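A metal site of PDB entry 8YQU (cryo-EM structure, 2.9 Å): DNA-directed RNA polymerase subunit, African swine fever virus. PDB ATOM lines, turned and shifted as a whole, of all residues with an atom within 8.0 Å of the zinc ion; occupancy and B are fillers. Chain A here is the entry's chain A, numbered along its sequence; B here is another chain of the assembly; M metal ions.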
ATOM      1  N   ILE A  98       6.834 -27.053  -6.110  1.00  0.00           N
ATOM      2  CA  ILE A  98       6.347 -25.803  -5.535  1.00  0.00           C
ATOM      3  C   ILE A  98       5.475 -25.092  -6.562  1.00  0.00           C
ATOM      4  O   ILE A  98       5.587 -25.317  -7.776  1.00  0.00           O
ATOM      5  CB  ILE A  98       7.505 -24.898  -5.080  1.00  0.00           C
ATOM      6  CG1 ILE A  98       8.345 -24.496  -6.296  1.00  0.00           C
ATOM      7  CG2 ILE A  98       8.360 -25.603  -4.042  1.00  0.00           C
ATOM      8  CD1 ILE A  98       9.357 -23.425  -6.002  1.00  0.00           C
ATOM      9  N   CYS A  99       4.596 -24.224  -6.075  1.00  0.00           N
ATOM     10  CA  CYS A  99       3.821 -23.367  -6.950  1.00  0.00           C
ATOM     11  C   CYS A  99       4.685 -22.228  -7.468  1.00  0.00           C
ATOM     12  O   CYS A  99       5.554 -21.719  -6.752  1.00  0.00           O
ATOM     13  CB  CYS A  99       2.604 -22.824  -6.206  1.00  0.00           C
ATOM     14  SG  CYS A  99       1.529 -21.762  -7.210  1.00  0.00           S
ATOM     15  N   LEU A 100       4.462 -21.845  -8.711  1.00  0.00           N
ATOM     16  CA  LEU A 100       5.259 -20.798  -9.346  1.00  0.00           C
ATOM     17  C   LEU A 100       4.742 -19.392  -9.065  1.00  0.00           C
ATOM     18  O   LEU A 100       5.335 -18.428  -9.551  1.00  0.00           O
ATOM     19  CB  LEU A 100       5.343 -21.025 -10.863  1.00  0.00           C
ATOM     20  CG  LEU A 100       6.520 -21.827 -11.427  1.00  0.00           C
ATOM     21  CD1 LEU A 100       6.786 -23.099 -10.627  1.00  0.00           C
ATOM     22  CD2 LEU A 100       6.288 -22.154 -12.902  1.00  0.00           C
ATOM     23  N   ASN A 101       3.656 -19.248  -8.309  1.00  0.00           N
ATOM     24  CA  ASN A 101       3.119 -17.941  -7.972  1.00  0.00           C
ATOM     25  C   ASN A 101       3.073 -17.624  -6.486  1.00  0.00           C
ATOM     26  O   ASN A 101       3.146 -16.444  -6.130  1.00  0.00           O
ATOM     27  CB  ASN A 101       1.697 -17.771  -8.541  1.00  0.00           C
ATOM     28  CG  ASN A 101       1.679 -17.651 -10.049  1.00  0.00           C
ATOM     29  OD1 ASN A 101       2.524 -16.972 -10.645  1.00  0.00           O
ATOM     30  ND2 ASN A 101       0.700 -18.286 -10.680  1.00  0.00           N
ATOM     31  N   CYS A 102       2.991 -18.631  -5.611  1.00  0.00           N
ATOM     32  CA  CYS A 102       2.988 -18.395  -4.169  1.00  0.00           C
ATOM     33  C   CYS A 102       4.104 -19.126  -3.452  1.00  0.00           C
ATOM     34  O   CYS A 102       4.395 -18.800  -2.290  1.00  0.00           O
ATOM     35  CB  CYS A 102       1.680 -18.852  -3.526  1.00  0.00           C
ATOM     36  SG  CYS A 102       1.474 -20.636  -3.657  1.00  0.00           S
ATOM     37  N   GLY A 103       4.712 -20.130  -4.073  1.00  0.00           N
ATOM     38  CA  GLY A 103       5.787 -20.889  -3.489  1.00  0.00           C
ATOM     39  C   GLY A 103       5.381 -22.054  -2.605  1.00  0.00           C
ATOM     40  O   GLY A 103       6.236 -22.892  -2.289  1.00  0.00           O
ATOM     41  N   ALA A 104       4.110 -22.154  -2.223  1.00  0.00           N
ATOM     42  CA  ALA A 104       3.697 -23.232  -1.335  1.00  0.00           C
ATOM     43  C   ALA A 104       3.825 -24.579  -2.049  1.00  0.00           C
ATOM     44  O   ALA A 104       3.688 -24.659  -3.273  1.00  0.00           O
ATOM     45  CB  ALA A 104       2.261 -23.018  -0.861  1.00  0.00           C
ATOM     46  N   PRO A 105       4.097 -25.656  -1.307  1.00  0.00           N
ATOM     47  CA  PRO A 105       4.173 -26.978  -1.951  1.00  0.00           C
ATOM     48  C   PRO A 105       2.832 -27.362  -2.546  1.00  0.00           C
ATOM     49  O   PRO A 105       1.771 -27.047  -1.998  1.00  0.00           O
ATOM     50  CB  PRO A 105       4.580 -27.911  -0.808  1.00  0.00           C
ATOM     51  CG  PRO A 105       4.043 -27.242   0.403  1.00  0.00           C
ATOM     52  CD  PRO A 105       4.167 -25.765   0.155  1.00  0.00           C
ATOM     53  N   ILE A 106       2.880 -28.048  -3.686  1.00  0.00           N
ATOM     54  CA  ILE A 106       1.667 -28.514  -4.349  1.00  0.00           C
ATOM     55  C   ILE A 106       1.298 -29.908  -3.896  1.00  0.00           C
ATOM     56  O   ILE A 106       0.163 -30.183  -3.512  1.00  0.00           O
ATOM     57  CB  ILE A 106       1.845 -28.430  -5.877  1.00  0.00           C
ATOM     58  CG1 ILE A 106       1.786 -26.976  -6.330  1.00  0.00           C
ATOM     59  CG2 ILE A 106       0.785 -29.250  -6.578  1.00  0.00           C
ATOM     60  CD1 ILE A 106       2.286 -26.758  -7.729  1.00  0.00           C
ATOM     61  N   LYS A 132      -2.392 -29.381 -11.378  1.00  0.00           N
ATOM     62  CA  LYS A 132      -2.852 -29.342 -10.004  1.00  0.00           C
ATOM     63  C   LYS A 132      -3.104 -27.907  -9.556  1.00  0.00           C
ATOM     64  O   LYS A 132      -2.370 -26.993  -9.933  1.00  0.00           O
ATOM     65  CB  LYS A 132      -1.863 -30.035  -9.071  1.00  0.00           C
ATOM     66  CG  LYS A 132      -1.793 -31.537  -9.266  1.00  0.00           C
ATOM     67  CD  LYS A 132      -0.816 -32.190  -8.306  1.00  0.00           C
ATOM     68  CE  LYS A 132      -0.880 -33.709  -8.416  1.00  0.00           C
ATOM     69  NZ  LYS A 132      -0.404 -34.198  -9.732  1.00  0.00           N
ATOM     70  N   GLN A 133      -4.130 -27.734  -8.740  1.00  0.00           N
ATOM     71  CA  GLN A 133      -4.585 -26.417  -8.323  1.00  0.00           C
ATOM     72  C   GLN A 133      -4.066 -26.103  -6.919  1.00  0.00           C
ATOM     73  O   GLN A 133      -4.267 -26.874  -5.985  1.00  0.00           O
ATOM     74  CB  GLN A 133      -6.114 -26.348  -8.359  1.00  0.00           C
ATOM     75  CG  GLN A 133      -6.711 -24.978  -8.088  1.00  0.00           C
ATOM     76  CD  GLN A 133      -6.936 -24.739  -6.607  1.00  0.00           C
ATOM     77  OE1 GLN A 133      -7.177 -25.672  -5.847  1.00  0.00           O
ATOM     78  NE2 GLN A 133      -6.861 -23.477  -6.205  1.00  0.00           N
ATOM     79  N   CYS A 134      -3.386 -24.964  -6.801  1.00  0.00           N
ATOM     80  CA  CYS A 134      -2.777 -24.581  -5.536  1.00  0.00           C
ATOM     81  C   CYS A 134      -3.829 -24.192  -4.504  1.00  0.00           C
ATOM     82  O   CYS A 134      -4.866 -23.608  -4.831  1.00  0.00           O
ATOM     83  CB  CYS A 134      -1.806 -23.417  -5.761  1.00  0.00           C
ATOM     84  SG  CYS A 134      -0.788 -23.067  -4.324  1.00  0.00           S
ATOM     85  N   TYR A 135      -3.539 -24.504  -3.246  1.00  0.00           N
ATOM     86  CA  TYR A 135      -4.513 -24.373  -2.171  1.00  0.00           C
ATOM     87  C   TYR A 135      -4.560 -22.995  -1.528  1.00  0.00           C
ATOM     88  O   TYR A 135      -5.459 -22.734  -0.715  1.00  0.00           O
ATOM     89  CB  TYR A 135      -4.237 -25.412  -1.080  1.00  0.00           C
ATOM     90  CG  TYR A 135      -4.543 -26.843  -1.476  1.00  0.00           C
ATOM     91  CD1 TYR A 135      -3.789 -27.488  -2.440  1.00  0.00           C
ATOM     92  CD2 TYR A 135      -5.594 -27.532  -0.887  1.00  0.00           C
ATOM     93  CE1 TYR A 135      -4.072 -28.794  -2.816  1.00  0.00           C
ATOM     94  CE2 TYR A 135      -5.887 -28.833  -1.246  1.00  0.00           C
ATOM     95  CZ  TYR A 135      -5.120 -29.460  -2.209  1.00  0.00           C
ATOM     96  OH  TYR A 135      -5.397 -30.755  -2.573  1.00  0.00           O
ATOM     97  N   VAL A 136      -3.636 -22.090  -1.853  1.00  0.00           N
ATOM     98  CA  VAL A 136      -3.538 -20.815  -1.155  1.00  0.00           C
ATOM     99  C   VAL A 136      -3.585 -19.603  -2.074  1.00  0.00           C
ATOM    100  O   VAL A 136      -3.920 -18.510  -1.600  1.00  0.00           O
ATOM    101  CB  VAL A 136      -2.275 -20.763  -0.269  1.00  0.00           C
ATOM    102  CG1 VAL A 136      -2.470 -21.620   0.971  1.00  0.00           C
ATOM    103  CG2 VAL A 136      -1.069 -21.238  -1.042  1.00  0.00           C
ATOM    104  N   CYS A 137      -3.259 -19.752  -3.358  1.00  0.00           N
ATOM    105  CA  CYS A 137      -3.311 -18.634  -4.286  1.00  0.00           C
ATOM    106  C   CYS A 137      -4.257 -18.873  -5.455  1.00  0.00           C
ATOM    107  O   CYS A 137      -4.532 -17.934  -6.214  1.00  0.00           O
ATOM    108  CB  CYS A 137      -1.905 -18.333  -4.823  1.00  0.00           C
ATOM    109  SG  CYS A 137      -1.332 -19.521  -6.038  1.00  0.00           S
ATOM    110  N   LYS A 138      -4.767 -20.098  -5.616  1.00  0.00           N
ATOM    111  CA  LYS A 138      -5.679 -20.454  -6.705  1.00  0.00           C
ATOM    112  C   LYS A 138      -4.994 -20.278  -8.068  1.00  0.00           C
ATOM    113  O   LYS A 138      -5.416 -19.467  -8.893  1.00  0.00           O
ATOM    114  CB  LYS A 138      -6.984 -19.659  -6.630  1.00  0.00           C
ATOM    115  CG  LYS A 138      -7.580 -19.556  -5.234  1.00  0.00           C
ATOM    116  CD  LYS A 138      -8.126 -20.884  -4.748  1.00  0.00           C
ATOM    117  CE  LYS A 138      -8.753 -20.736  -3.373  1.00  0.00           C
ATOM    118  NZ  LYS A 138      -9.976 -19.898  -3.408  1.00  0.00           N
ATOM    119  N   ALA A 139      -3.915 -21.031  -8.285  1.00  0.00           N
ATOM    120  CA  ALA A 139      -3.183 -21.010  -9.536  1.00  0.00           C
ATOM    121  C   ALA A 139      -2.962 -22.419 -10.045  1.00  0.00           C
ATOM    122  O   ALA A 139      -2.734 -23.355  -9.267  1.00  0.00           O
ATOM    123  CB  ALA A 139      -1.835 -20.300  -9.389  1.00  0.00           C
ATOM    124  N   VAL A 140      -3.032 -22.576 -11.374  1.00  0.00           N
ATOM    125  CA  VAL A 140      -2.819 -23.873 -12.007  1.00  0.00           C
ATOM    126  C   VAL A 140      -1.335 -24.040 -12.301  1.00  0.00           C
ATOM    127  O   VAL A 140      -0.708 -23.172 -12.915  1.00  0.00           O
ATOM    128  CB  VAL A 140      -3.663 -23.989 -13.289  1.00  0.00           C
ATOM    129  CG1 VAL A 140      -3.492 -25.361 -13.922  1.00  0.00           C
ATOM    130  CG2 VAL A 140      -5.128 -23.699 -12.988  1.00  0.00           C
ATOM    131  N   HIS A 141      -0.779 -25.170 -11.883  1.00  0.00           N
ATOM    132  CA  HIS A 141       0.641 -25.426 -12.064  1.00  0.00           C
ATOM    133  C   HIS A 141       0.933 -25.818 -13.506  1.00  0.00           C
ATOM    134  O   HIS A 141       0.411 -26.840 -13.965  1.00  0.00           O
ATOM    135  CB  HIS A 141       1.117 -26.517 -11.119  1.00  0.00           C
ATOM    136  CG  HIS A 141       2.590 -26.766 -11.153  1.00  0.00           C
ATOM    137  ND1 HIS A 141       3.505 -25.877 -10.629  1.00  0.00           N
ATOM    138  CD2 HIS A 141       3.306 -27.806 -11.629  1.00  0.00           C
ATOM    139  CE1 HIS A 141       4.728 -26.359 -10.791  1.00  0.00           C
ATOM    140  NE2 HIS A 141       4.635 -27.524 -11.402  1.00  0.00           N
ATOM    141  N   ARG A 176      10.961 -17.577  -2.696  1.00  0.00           N
ATOM    142  CA  ARG A 176       9.683 -17.530  -2.007  1.00  0.00           C
ATOM    143  C   ARG A 176       9.346 -18.820  -1.258  1.00  0.00           C
ATOM    144  O   ARG A 176       8.284 -18.895  -0.634  1.00  0.00           O
ATOM    145  CB  ARG A 176       8.569 -17.181  -3.019  1.00  0.00           C
ATOM    146  CG  ARG A 176       7.160 -16.995  -2.497  1.00  0.00           C
ATOM    147  CD  ARG A 176       6.202 -16.597  -3.568  1.00  0.00           C
ATOM    148  NE  ARG A 176       6.575 -15.259  -4.036  1.00  0.00           N
ATOM    149  CZ  ARG A 176       7.064 -14.956  -5.229  1.00  0.00           C
ATOM    150  NH1 ARG A 176       7.266 -15.882  -6.156  1.00  0.00           N
ATOM    151  NH2 ARG A 176       7.384 -13.700  -5.486  1.00  0.00           N
ATOM    152  N   LEU B 117       3.974 -18.418   4.403  1.00  0.00           N
ATOM    153  CA  LEU B 117       4.467 -18.134   3.063  1.00  0.00           C
ATOM    154  C   LEU B 117       5.792 -17.394   3.176  1.00  0.00           C
ATOM    155  O   LEU B 117       6.339 -17.240   4.276  1.00  0.00           O
ATOM    156  CB  LEU B 117       3.448 -17.327   2.256  1.00  0.00           C
ATOM    157  CG  LEU B 117       2.151 -18.040   1.887  1.00  0.00           C
ATOM    158  CD1 LEU B 117       1.136 -17.066   1.293  1.00  0.00           C
ATOM    159  CD2 LEU B 117       2.412 -19.194   0.925  1.00  0.00           C
HETATM  160 ZN    ZN M   1       0.129 -21.243  -5.426  1.00  0.00          ZN
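The zinc ion is bound by the side-chain sulfur (SG) of Cys 102, at 2.3 Å.
SG of Cys 134 is bound to the zinc ion (2.3 Å).
The side-chain sulfur (SG) of Cys 99 binds the zinc ion (2.3 Å).
SG of Cys 137 binds the zinc ion.
The zinc ion has four donor atoms within binding distance.
Of the 21 residues printed, 4 come within 4 Å of the zinc ion.
The nearest printed residue that does not touch the zinc ion is Ala 139 (4.5 Å).
SG of Cys 102 sits close to N of Ala 104 (3.4 Å).
The backbone carbonyl oxygen (O) of Ala 139 sits at hydrogen-bond distance from the backbone NH (N) of Cys 134, 3.0 Å away.
The backbone NH of Asn 101 sits close to the side-chain sulfur of Cys 99, at 3.5 Å.
O of Ala 104 is in hydrogen-bond range of N of Cys 99, 3.0 Å away.
The side-chain sulfur (SG) of Cys 137 lies close to the backbone NH (N) of Ala 139, at 3.7 Å.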
